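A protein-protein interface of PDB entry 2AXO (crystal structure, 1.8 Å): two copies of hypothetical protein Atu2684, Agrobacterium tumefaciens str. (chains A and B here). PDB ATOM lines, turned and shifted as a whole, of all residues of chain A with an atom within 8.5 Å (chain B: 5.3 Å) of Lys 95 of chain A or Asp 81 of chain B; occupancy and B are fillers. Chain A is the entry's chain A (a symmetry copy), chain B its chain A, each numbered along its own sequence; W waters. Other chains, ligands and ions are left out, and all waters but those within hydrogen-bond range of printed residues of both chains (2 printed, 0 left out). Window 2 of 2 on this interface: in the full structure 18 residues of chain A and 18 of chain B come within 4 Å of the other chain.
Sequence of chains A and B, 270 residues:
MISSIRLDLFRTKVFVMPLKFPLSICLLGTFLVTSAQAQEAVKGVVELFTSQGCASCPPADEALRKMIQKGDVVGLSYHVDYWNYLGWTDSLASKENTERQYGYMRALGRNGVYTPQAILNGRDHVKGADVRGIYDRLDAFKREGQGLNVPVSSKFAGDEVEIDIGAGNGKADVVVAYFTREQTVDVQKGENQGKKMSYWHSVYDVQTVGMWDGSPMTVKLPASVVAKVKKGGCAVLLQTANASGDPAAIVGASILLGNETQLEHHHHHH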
ATOM      1  N   HIS A  79      -9.476  -9.079  21.480  1.00  0.00           N
ATOM      2  CA  HIS A  79      -9.690  -7.638  21.525  1.00  0.00           C
ATOM      3  C   HIS A  79      -9.199  -7.084  22.856  1.00  0.00           C
ATOM      4  O   HIS A  79      -9.662  -7.503  23.918  1.00  0.00           O
ATOM      5  CB  HIS A  79     -11.172  -7.310  21.333  1.00  0.00           C
ATOM      6  CG  HIS A  79     -11.654  -7.497  19.928  1.00  0.00           C
ATOM      7  ND1 HIS A  79     -11.736  -8.733  19.325  1.00  0.00           N
ATOM      8  CD2 HIS A  79     -12.073  -6.599  19.004  1.00  0.00           C
ATOM      9  CE1 HIS A  79     -12.188  -8.590  18.091  1.00  0.00           C
ATOM     10  NE2 HIS A  79     -12.399  -7.305  17.871  1.00  0.00           N
ATOM     11  N   VAL A  80      -8.256  -6.146  22.791  1.00  0.00           N
ATOM     12  CA  VAL A  80      -7.692  -5.525  23.989  1.00  0.00           C
ATOM     13  C   VAL A  80      -8.562  -4.363  24.462  1.00  0.00           C
ATOM     14  O   VAL A  80      -9.315  -3.782  23.682  1.00  0.00           O
ATOM     15  CB  VAL A  80      -6.253  -5.024  23.727  1.00  0.00           C
ATOM     16  CG1 VAL A  80      -5.354  -6.209  23.420  1.00  0.00           C
ATOM     17  CG2 VAL A  80      -6.241  -4.029  22.571  1.00  0.00           C
ATOM     18  N   ASP A  81      -8.458  -4.016  25.741  1.00  0.00           N
ATOM     19  CA  ASP A  81      -9.283  -2.941  26.275  1.00  0.00           C
ATOM     20  C   ASP A  81      -8.636  -1.564  26.313  1.00  0.00           C
ATOM     21  O   ASP A  81      -9.307  -0.576  26.608  1.00  0.00           O
ATOM     22  CB  ASP A  81      -9.771  -3.308  27.685  1.00  0.00           C
ATOM     23  CG  ASP A  81      -8.646  -3.350  28.703  1.00  0.00           C
ATOM     24  OD1 ASP A  81      -7.464  -3.248  28.310  1.00  0.00           O
ATOM     25  OD2 ASP A  81      -8.945  -3.491  29.907  1.00  0.00           O
ATOM     26  N   TYR A  82      -7.351  -1.473  25.992  1.00  0.00           N
ATOM     27  CA  TYR A  82      -6.706  -0.175  26.067  1.00  0.00           C
ATOM     28  C   TYR A  82      -6.949   0.804  24.922  1.00  0.00           C
ATOM     29  O   TYR A  82      -6.207   1.769  24.750  1.00  0.00           O
ATOM     30  CB  TYR A  82      -5.205  -0.346  26.332  1.00  0.00           C
ATOM     31  CG  TYR A  82      -4.441  -1.246  25.389  1.00  0.00           C
ATOM     32  CD1 TYR A  82      -4.120  -0.828  24.101  1.00  0.00           C
ATOM     33  CD2 TYR A  82      -3.943  -2.471  25.828  1.00  0.00           C
ATOM     34  CE1 TYR A  82      -3.305  -1.601  23.276  1.00  0.00           C
ATOM     35  CE2 TYR A  82      -3.133  -3.252  25.018  1.00  0.00           C
ATOM     36  CZ  TYR A  82      -2.811  -2.811  23.747  1.00  0.00           C
ATOM     37  OH  TYR A  82      -1.963  -3.557  22.965  1.00  0.00           O
ATOM     38  N   ASN A  84     -10.316   1.672  24.458  1.00  0.00           N
ATOM     39  CA  ASN A  84     -11.638   2.157  24.823  1.00  0.00           C
ATOM     40  C   ASN A  84     -11.488   3.489  25.538  1.00  0.00           C
ATOM     41  O   ASN A  84     -10.526   3.704  26.274  1.00  0.00           O
ATOM     42  CB  ASN A  84     -12.347   1.162  25.749  1.00  0.00           C
ATOM     43  CG  ASN A  84     -12.372  -0.245  25.189  1.00  0.00           C
ATOM     44  OD1 ASN A  84     -12.628  -0.452  24.003  1.00  0.00           O
ATOM     45  ND2 ASN A  84     -12.115  -1.225  26.046  1.00  0.00           N
ATOM     46  N   LEU A  92     -16.293  -6.306  22.499  1.00  0.00           N
ATOM     47  CA  LEU A  92     -15.552  -7.545  22.302  1.00  0.00           C
ATOM     48  C   LEU A  92     -14.245  -7.557  23.082  1.00  0.00           C
ATOM     49  O   LEU A  92     -13.559  -8.574  23.135  1.00  0.00           O
ATOM     50  CB  LEU A  92     -15.253  -7.751  20.816  1.00  0.00           C
ATOM     51  CG  LEU A  92     -16.411  -8.220  19.939  1.00  0.00           C
ATOM     52  CD1 LEU A  92     -16.019  -8.123  18.475  1.00  0.00           C
ATOM     53  CD2 LEU A  92     -16.770  -9.650  20.312  1.00  0.00           C
ATOM     54  N   ALA A  93     -13.905  -6.424  23.687  1.00  0.00           N
ATOM     55  CA  ALA A  93     -12.666  -6.315  24.448  1.00  0.00           C
ATOM     56  C   ALA A  93     -12.832  -6.760  25.891  1.00  0.00           C
ATOM     57  O   ALA A  93     -13.946  -6.827  26.410  1.00  0.00           O
ATOM     58  CB  ALA A  93     -12.156  -4.881  24.410  1.00  0.00           C
ATOM     59  N   SER A  94     -11.712  -7.066  26.537  1.00  0.00           N
ATOM     60  CA  SER A  94     -11.735  -7.476  27.930  1.00  0.00           C
ATOM     61  C   SER A  94     -10.362  -7.282  28.556  1.00  0.00           C
ATOM     62  O   SER A  94      -9.333  -7.288  27.872  1.00  0.00           O
ATOM     63  CB  SER A  94     -12.158  -8.942  28.066  1.00  0.00           C
ATOM     64  OG  SER A  94     -11.081  -9.813  27.792  1.00  0.00           O
ATOM     65  N   LYS A  95     -10.365  -7.115  29.870  1.00  0.00           N
ATOM     66  CA  LYS A  95      -9.148  -6.920  30.637  1.00  0.00           C
ATOM     67  C   LYS A  95      -8.322  -8.202  30.589  1.00  0.00           C
ATOM     68  O   LYS A  95      -7.095  -8.161  30.539  1.00  0.00           O
ATOM     69  CB  LYS A  95      -9.520  -6.564  32.080  1.00  0.00           C
ATOM     70  CG  LYS A  95      -8.434  -5.868  32.879  1.00  0.00           C
ATOM     71  CD  LYS A  95      -7.437  -6.845  33.462  1.00  0.00           C
ATOM     72  CE  LYS A  95      -6.401  -6.122  34.313  1.00  0.00           C
ATOM     73  NZ  LYS A  95      -5.610  -5.133  33.520  1.00  0.00           N
ATOM     74  N   GLU A  96      -9.009  -9.340  30.592  1.00  0.00           N
ATOM     75  CA  GLU A  96      -8.348 -10.641  30.548  1.00  0.00           C
ATOM     76  C   GLU A  96      -7.545 -10.809  29.262  1.00  0.00           C
ATOM     77  O   GLU A  96      -6.451 -11.369  29.276  1.00  0.00           O
ATOM     78  CB  GLU A  96      -9.381 -11.766  30.670  1.00  0.00           C
ATOM     79  CG  GLU A  96     -10.012 -11.898  32.058  1.00  0.00           C
ATOM     80  CD  GLU A  96     -10.761 -10.650  32.487  1.00  0.00           C
ATOM     81  OE1 GLU A  96     -11.670 -10.215  31.750  1.00  0.00           O
ATOM     82  OE2 GLU A  96     -10.443 -10.100  33.564  1.00  0.00           O
ATOM     83  N   ASN A  97      -8.090 -10.329  28.149  1.00  0.00           N
ATOM     84  CA  ASN A  97      -7.386 -10.431  26.880  1.00  0.00           C
ATOM     85  C   ASN A  97      -6.127  -9.593  26.921  1.00  0.00           C
ATOM     86  O   ASN A  97      -5.074 -10.011  26.447  1.00  0.00           O
ATOM     87  CB  ASN A  97      -8.257  -9.946  25.727  1.00  0.00           C
ATOM     88  CG  ASN A  97      -9.312 -10.942  25.344  1.00  0.00           C
ATOM     89  OD1 ASN A  97      -9.277 -12.086  25.784  1.00  0.00           O
ATOM     90  ND2 ASN A  97     -10.256 -10.519  24.509  1.00  0.00           N
ATOM     91  N   THR A  98      -6.242  -8.394  27.474  1.00  0.00           N
ATOM     92  CA  THR A  98      -5.086  -7.526  27.558  1.00  0.00           C
ATOM     93  C   THR A  98      -4.037  -8.175  28.461  1.00  0.00           C
ATOM     94  O   THR A  98      -2.846  -8.149  28.155  1.00  0.00           O
ATOM     95  CB  THR A  98      -5.465  -6.132  28.099  1.00  0.00           C
ATOM     96  OG1 THR A  98      -6.527  -5.586  27.305  1.00  0.00           O
ATOM     97  CG2 THR A  98      -4.266  -5.192  28.030  1.00  0.00           C
ATOM     98  N   GLU A  99      -4.474  -8.779  29.560  1.00  0.00           N
ATOM     99  CA  GLU A  99      -3.531  -9.434  30.461  1.00  0.00           C
ATOM    100  C   GLU A  99      -2.758 -10.545  29.760  1.00  0.00           C
ATOM    101  O   GLU A  99      -1.585 -10.776  30.063  1.00  0.00           O
ATOM    102  CB  GLU A  99      -4.257  -9.990  31.687  1.00  0.00           C
ATOM    103  CG  GLU A  99      -4.849  -8.897  32.559  1.00  0.00           C
ATOM    104  CD  GLU A  99      -5.399  -9.424  33.861  1.00  0.00           C
ATOM    105  OE1 GLU A  99      -6.221 -10.363  33.823  1.00  0.00           O
ATOM    106  OE2 GLU A  99      -5.014  -8.892  34.925  1.00  0.00           O
ATOM    107  N   ARG A 100      -3.404 -11.229  28.820  1.00  0.00           N
ATOM    108  CA  ARG A 100      -2.717 -12.292  28.092  1.00  0.00           C
ATOM    109  C   ARG A 100      -1.618 -11.668  27.235  1.00  0.00           C
ATOM    110  O   ARG A 100      -0.524 -12.216  27.136  1.00  0.00           O
ATOM    111  CB  ARG A 100      -3.700 -13.089  27.221  1.00  0.00           C
ATOM    112  CG  ARG A 100      -3.069 -14.268  26.472  1.00  0.00           C
ATOM    113  CD  ARG A 100      -4.154 -15.180  25.907  1.00  0.00           C
ATOM    114  NE  ARG A 100      -3.637 -16.311  25.128  1.00  0.00           N
ATOM    115  CZ  ARG A 100      -3.015 -17.367  25.646  1.00  0.00           C
ATOM    116  NH1 ARG A 100      -2.810 -17.457  26.956  1.00  0.00           N
ATOM    117  NH2 ARG A 100      -2.621 -18.351  24.856  1.00  0.00           N
ATOM    118  N   GLN A 101      -1.887 -10.518  26.621  1.00  0.00           N
ATOM    119  CA  GLN A 101      -0.850  -9.890  25.817  1.00  0.00           C
ATOM    120  C   GLN A 101       0.306  -9.470  26.733  1.00  0.00           C
ATOM    121  O   GLN A 101       1.461  -9.462  26.309  1.00  0.00           O
ATOM    122  CB  GLN A 101      -1.395  -8.685  25.046  1.00  0.00           C
ATOM    123  CG  GLN A 101      -0.374  -8.025  24.129  1.00  0.00           C
ATOM    124  CD  GLN A 101      -0.968  -6.874  23.334  1.00  0.00           C
ATOM    125  OE1 GLN A 101      -1.808  -6.127  23.838  1.00  0.00           O
ATOM    126  NE2 GLN A 101      -0.519  -6.714  22.094  1.00  0.00           N
ATOM    127  N   TYR A 102       0.000  -9.131  27.987  1.00  0.00           N
ATOM    128  CA  TYR A 102       1.045  -8.751  28.941  1.00  0.00           C
ATOM    129  C   TYR A 102       1.888  -9.979  29.264  1.00  0.00           C
ATOM    130  O   TYR A 102       3.113  -9.902  29.364  1.00  0.00           O
ATOM    131  CB  TYR A 102       0.447  -8.216  30.250  1.00  0.00           C
ATOM    132  CG  TYR A 102      -0.331  -6.932  30.118  1.00  0.00           C
ATOM    133  CD1 TYR A 102       0.023  -5.972  29.173  1.00  0.00           C
ATOM    134  CD2 TYR A 102      -1.389  -6.651  30.980  1.00  0.00           C
ATOM    135  CE1 TYR A 102      -0.658  -4.761  29.089  1.00  0.00           C
ATOM    136  CE2 TYR A 102      -2.071  -5.441  30.906  1.00  0.00           C
ATOM    137  CZ  TYR A 102      -1.695  -4.501  29.958  1.00  0.00           C
ATOM    138  OH  TYR A 102      -2.346  -3.290  29.898  1.00  0.00           O
ATOM    139  N   MET A 105       4.222 -10.387  26.569  1.00  0.00           N
ATOM    140  CA  MET A 105       5.248  -9.347  26.603  1.00  0.00           C
ATOM    141  C   MET A 105       6.375  -9.795  27.525  1.00  0.00           C
ATOM    142  O   MET A 105       7.545  -9.774  27.151  1.00  0.00           O
ATOM    143  CB  MET A 105       4.673  -8.028  27.126  1.00  0.00           C
ATOM    144  CG  MET A 105       5.735  -6.958  27.402  1.00  0.00           C
ATOM    145  SD  MET A 105       5.047  -5.455  28.420  1.00  0.00           S
ATOM    146  CE  MET A 105       5.018  -6.311  30.142  1.00  0.00           C
ATOM    147  N   ARG A 106       6.011 -10.195  28.738  1.00  0.00           N
ATOM    148  CA  ARG A 106       6.998 -10.637  29.709  1.00  0.00           C
ATOM    149  C   ARG A 106       7.772 -11.855  29.231  1.00  0.00           C
ATOM    150  O   ARG A 106       9.000 -11.858  29.266  1.00  0.00           O
ATOM    151  CB  ARG A 106       6.326 -10.943  31.046  1.00  0.00           C
ATOM    152  CG  ARG A 106       5.664  -9.736  31.690  1.00  0.00           C
ATOM    153  CD  ARG A 106       5.283 -10.035  33.130  1.00  0.00           C
ATOM    154  NE  ARG A 106       4.176 -10.977  33.247  1.00  0.00           N
ATOM    155  CZ  ARG A 106       2.896 -10.645  33.114  1.00  0.00           C
ATOM    156  NH1 ARG A 106       2.556  -9.387  32.857  1.00  0.00           N
ATOM    157  NH2 ARG A 106       1.954 -11.566  33.253  1.00  0.00           N
ATOM    158  N   TYR A 204     -13.665 -14.491  24.006  1.00  0.00           N
ATOM    159  CA  TYR A 204     -14.351 -13.833  25.113  1.00  0.00           C
ATOM    160  C   TYR A 204     -14.092 -14.498  26.458  1.00  0.00           C
ATOM    161  O   TYR A 204     -14.534 -14.002  27.496  1.00  0.00           O
ATOM    162  CB  TYR A 204     -15.857 -13.770  24.862  1.00  0.00           C
ATOM    163  CG  TYR A 204     -16.533 -15.112  24.753  1.00  0.00           C
ATOM    164  CD1 TYR A 204     -16.712 -15.724  23.513  1.00  0.00           C
ATOM    165  CD2 TYR A 204     -17.018 -15.759  25.886  1.00  0.00           C
ATOM    166  CE1 TYR A 204     -17.366 -16.947  23.404  1.00  0.00           C
ATOM    167  CE2 TYR A 204     -17.669 -16.983  25.790  1.00  0.00           C
ATOM    168  CZ  TYR A 204     -17.844 -17.570  24.546  1.00  0.00           C
ATOM    169  OH  TYR A 204     -18.511 -18.769  24.448  1.00  0.00           O
ATOM    170  N   HIS B  79       2.972   3.682  38.908  1.00  0.00           N
ATOM    171  CA  HIS B  79       3.314   2.275  38.747  1.00  0.00           C
ATOM    172  C   HIS B  79       2.220   1.562  37.962  1.00  0.00           C
ATOM    173  O   HIS B  79       1.058   1.557  38.371  1.00  0.00           O
ATOM    174  CB  HIS B  79       3.501   1.609  40.111  1.00  0.00           C
ATOM    175  CG  HIS B  79       4.769   2.000  40.805  1.00  0.00           C
ATOM    176  ND1 HIS B  79       5.000   3.276  41.273  1.00  0.00           N
ATOM    177  CD2 HIS B  79       5.878   1.283  41.104  1.00  0.00           C
ATOM    178  CE1 HIS B  79       6.197   3.327  41.833  1.00  0.00           C
ATOM    179  NE2 HIS B  79       6.750   2.132  41.743  1.00  0.00           N
ATOM    180  N   VAL B  80       2.598   0.970  36.831  1.00  0.00           N
ATOM    181  CA  VAL B  80       1.654   0.249  35.977  1.00  0.00           C
ATOM    182  C   VAL B  80       1.470  -1.188  36.458  1.00  0.00           C
ATOM    183  O   VAL B  80       2.333  -1.739  37.137  1.00  0.00           O
ATOM    184  CB  VAL B  80       2.129   0.248  34.506  1.00  0.00           C
ATOM    185  CG1 VAL B  80       2.150   1.674  33.980  1.00  0.00           C
ATOM    186  CG2 VAL B  80       3.515  -0.382  34.397  1.00  0.00           C
ATOM    187  N   ASP B  81       0.346  -1.800  36.103  1.00  0.00           N
ATOM    188  CA  ASP B  81       0.081  -3.160  36.556  1.00  0.00           C
ATOM    189  C   ASP B  81       0.464  -4.268  35.585  1.00  0.00           C
ATOM    190  O   ASP B  81       0.414  -5.444  35.942  1.00  0.00           O
ATOM    191  CB  ASP B  81      -1.401  -3.308  36.929  1.00  0.00           C
ATOM    192  CG  ASP B  81      -2.323  -3.212  35.727  1.00  0.00           C
ATOM    193  OD1 ASP B  81      -1.848  -2.881  34.620  1.00  0.00           O
ATOM    194  OD2 ASP B  81      -3.535  -3.465  35.890  1.00  0.00           O
ATOM    195  N   TYR B  82       0.874  -3.917  34.372  1.00  0.00           N
ATOM    196  CA  TYR B  82       1.199  -4.962  33.418  1.00  0.00           C
ATOM    197  C   TYR B  82       2.553  -5.651  33.558  1.00  0.00           C
ATOM    198  O   TYR B  82       3.029  -6.298  32.626  1.00  0.00           O
ATOM    199  CB  TYR B  82       0.987  -4.455  31.987  1.00  0.00           C
ATOM    200  CG  TYR B  82       1.687  -3.172  31.604  1.00  0.00           C
ATOM    201  CD1 TYR B  82       3.058  -3.149  31.361  1.00  0.00           C
ATOM    202  CD2 TYR B  82       0.958  -2.008  31.374  1.00  0.00           C
ATOM    203  CE1 TYR B  82       3.684  -2.000  30.881  1.00  0.00           C
ATOM    204  CE2 TYR B  82       1.567  -0.856  30.900  1.00  0.00           C
ATOM    205  CZ  TYR B  82       2.926  -0.858  30.648  1.00  0.00           C
ATOM    206  OH  TYR B  82       3.521   0.264  30.124  1.00  0.00           O
ATOM    207  N   TRP B  83       3.162  -5.527  34.732  1.00  0.00           N
ATOM    208  CA  TRP B  83       4.438  -6.179  34.997  1.00  0.00           C
ATOM    209  C   TRP B  83       4.270  -7.150  36.152  1.00  0.00           C
ATOM    210  O   TRP B  83       5.230  -7.775  36.603  1.00  0.00           O
ATOM    211  CB  TRP B  83       5.527  -5.157  35.333  1.00  0.00           C
ATOM    212  CG  TRP B  83       6.074  -4.476  34.133  1.00  0.00           C
ATOM    213  CD1 TRP B  83       5.789  -3.210  33.701  1.00  0.00           C
ATOM    214  CD2 TRP B  83       6.993  -5.027  33.185  1.00  0.00           C
ATOM    215  NE1 TRP B  83       6.476  -2.940  32.545  1.00  0.00           N
ATOM    216  CE2 TRP B  83       7.224  -4.038  32.205  1.00  0.00           C
ATOM    217  CE3 TRP B  83       7.644  -6.262  33.068  1.00  0.00           C
ATOM    218  CZ2 TRP B  83       8.087  -4.242  31.120  1.00  0.00           C
ATOM    219  CZ3 TRP B  83       8.500  -6.469  31.986  1.00  0.00           C
ATOM    220  CH2 TRP B  83       8.712  -5.461  31.029  1.00  0.00           C
ATOM    221  N   ASN B  84       3.038  -7.271  36.631  1.00  0.00           N
ATOM    222  CA  ASN B  84       2.743  -8.178  37.729  1.00  0.00           C
ATOM    223  C   ASN B  84       2.434  -9.552  37.158  1.00  0.00           C
ATOM    224  O   ASN B  84       1.846  -9.669  36.084  1.00  0.00           O
ATOM    225  CB  ASN B  84       1.538  -7.683  38.537  1.00  0.00           C
ATOM    226  CG  ASN B  84       1.685  -6.243  38.986  1.00  0.00           C
ATOM    227  OD1 ASN B  84       2.750  -5.826  39.439  1.00  0.00           O
ATOM    228  ND2 ASN B  84       0.607  -5.478  38.872  1.00  0.00           N
ATOM    229  N   ALA B  93       1.325  -0.558  42.201  1.00  0.00           N
ATOM    230  CA  ALA B  93       0.699  -0.507  40.886  1.00  0.00           C
ATOM    231  C   ALA B  93      -0.817  -0.502  40.966  1.00  0.00           C
ATOM    232  O   ALA B  93      -1.400  -0.878  41.982  1.00  0.00           O
ATOM    233  CB  ALA B  93       1.163  -1.688  40.042  1.00  0.00           C
ATOM    234  N   SER B  94      -1.455  -0.070  39.883  1.00  0.00           N
ATOM    235  CA  SER B  94      -2.906  -0.044  39.825  1.00  0.00           C
ATOM    236  C   SER B  94      -3.372  -0.002  38.377  1.00  0.00           C
ATOM    237  O   SER B  94      -2.655   0.460  37.482  1.00  0.00           O
ATOM    238  CB  SER B  94      -3.467   1.164  40.580  1.00  0.00           C
ATOM    239  OG  SER B  94      -3.381   2.339  39.800  1.00  0.00           O
ATOM    240  N   LYS B  95      -4.586  -0.486  38.165  1.00  0.00           N
ATOM    241  CA  LYS B  95      -5.194  -0.523  36.848  1.00  0.00           C
ATOM    242  C   LYS B  95      -5.454   0.907  36.383  1.00  0.00           C
ATOM    243  O   LYS B  95      -5.322   1.221  35.202  1.00  0.00           O
ATOM    244  CB  LYS B  95      -6.502  -1.317  36.925  1.00  0.00           C
ATOM    245  CG  LYS B  95      -7.012  -1.863  35.604  1.00  0.00           C
ATOM    246  CD  LYS B  95      -7.782  -0.827  34.816  1.00  0.00           C
ATOM    247  CE  LYS B  95      -8.336  -1.424  33.529  1.00  0.00           C
ATOM    248  NZ  LYS B  95      -7.255  -1.925  32.627  1.00  0.00           N
ATOM    249  N   THR B  98      -2.396   2.440  34.845  1.00  0.00           N
ATOM    250  CA  THR B  98      -2.168   1.933  33.508  1.00  0.00           C
ATOM    251  C   THR B  98      -3.151   2.600  32.546  1.00  0.00           C
ATOM    252  O   THR B  98      -2.779   2.981  31.437  1.00  0.00           O
ATOM    253  CB  THR B  98      -2.323   0.400  33.451  1.00  0.00           C
ATOM    254  OG1 THR B  98      -1.474  -0.202  34.439  1.00  0.00           O
ATOM    255  CG2 THR B  98      -1.926  -0.124  32.076  1.00  0.00           C
HETATM  256  O   HOH W   1      -5.905  -2.922  30.510  1.00  0.00           O
HETATM  257  O   HOH W   2      -3.775  -3.304  32.753  1.00  0.00           O
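The side-chain amino group of Lys 95 of chain B lies within salt-bridge range of the side-chain carboxylate of Asp 81 of chain A, 3.6 Å away. The backbone carbonyl oxygen of Asn 84 of chain B lies close to the guanidinium group of Arg 106 of chain A, 3.3 Å away. The backbone carbonyl oxygen (O) of Tyr 82 of chain B is in hydrogen-bond range of the guanidinium group (NH1) of Arg 106 of chain A (3.1 Å). NZ of Lys 95 of chain A lies within salt-bridge range of OD2 of Asp 81 of chain B (3.6 Å).
The side-chain carboxylate (OD1) of Asp 81 of chain A sits at hydrogen-bond distance from the side-chain hydroxyl (OG1) of Thr 98 of chain A. O of Asp 81 of chain A is in hydrogen-bond range of ND2 of Asn 84 of chain A (2.9 Å). The backbone carbonyl oxygen (O) of Asp 81 of chain B sits at hydrogen-bond distance from the side-chain amide nitrogen (ND2) of Asn 84 of chain B, at 2.9 Å. O of Ser 94 of chain B is in hydrogen-bond range of OG1 of Thr 98 of chain B, at 3.3 Å. The side-chain carboxylate of Asp 81 of chain B sits at hydrogen-bond distance from the side-chain hydroxyl of Thr 98 of chain B.
Among the printed residues, merely in contact across the chains: Met 105 of chain A with Tyr 82 of chain B (3.2 Å), Tyr 102 of chain A with Tyr 82 of chain B (3.3 Å), Lys 95 of chain A with Lys 95 of chain B (3.7 Å), Met 105 of chain A with Trp 83 of chain B (3.8 Å) and Tyr 102 of chain A with Thr 98 of chain B (3.9 Å).
Val 80 of chain A touches none of the printed residues of chain B. Printed residues of chain B within 4 Å of Asp 81 of chain A: Lys 95. Of the printed residues of chain B, Lys 95 of chain A touches Asp 81 and Lys 95. Of the printed residues of chain B, Tyr 102 of chain A touches Tyr 82 and Thr 98. Asp 81 of chain B touches just one residue of chain A: Lys 95 (3.6 Å). Of the printed residues of chain A, Lys 95 of chain B touches Asp 81 and Lys 95. The nearest printed residue of chain B that does not touch Lys 95 of chain A is Thr 98 of chain B (6.4 Å). The nearest residue of chain A that does not touch Asp 81 of chain B is Tyr 102 of chain A (4.5 Å). The nearest printed residue of chain B that does not touch Asp 81 of chain A is Thr 98 of chain B (7.4 Å).
Hydrophobic or aromatic side chains of chain B that line the printed part of chain A: Tyr 82 and Trp 83. Of the 19 printed residues of chain A, 5 touch a printed residue of chain B. Hydrophobic or aromatic side chains of chain A that line the printed part of chain B: Tyr 102 and Met 105. Along chain A the printed residues that touch a printed residue of chain B span positions 81 to 106.
Asp 81 of chain A touches Lys 95 of chain B, and with the chains exchanged Lys 95 of chain A touches Asp 81 of chain B. Lys 95 of chain B touches its own counterpart, Lys 95 of chain A. Positions printed for both chains: 79, 80, 81, 82, 84, 93, 94, 95 and 98. Of the 9 pairs that touch across the chains among the printed residues, 3 have their exchanged pair printed and touching as well.
Water W2 lies within hydrogen-bond range of the side-chain amino group (NZ) of Lys 95 of chain A (2.7 Å), the side-chain carboxylate (OD1) of Asp 81 of chain B (2.7 Å) and the side-chain hydroxyl (OH) of Tyr 102 of chain A (3.2 Å). Water W1 bridges the side-chain amino group of Lys 95 of chain B (2.7 Å) and the side-chain carboxylate of Asp 81 of chain A (2.7 Å).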
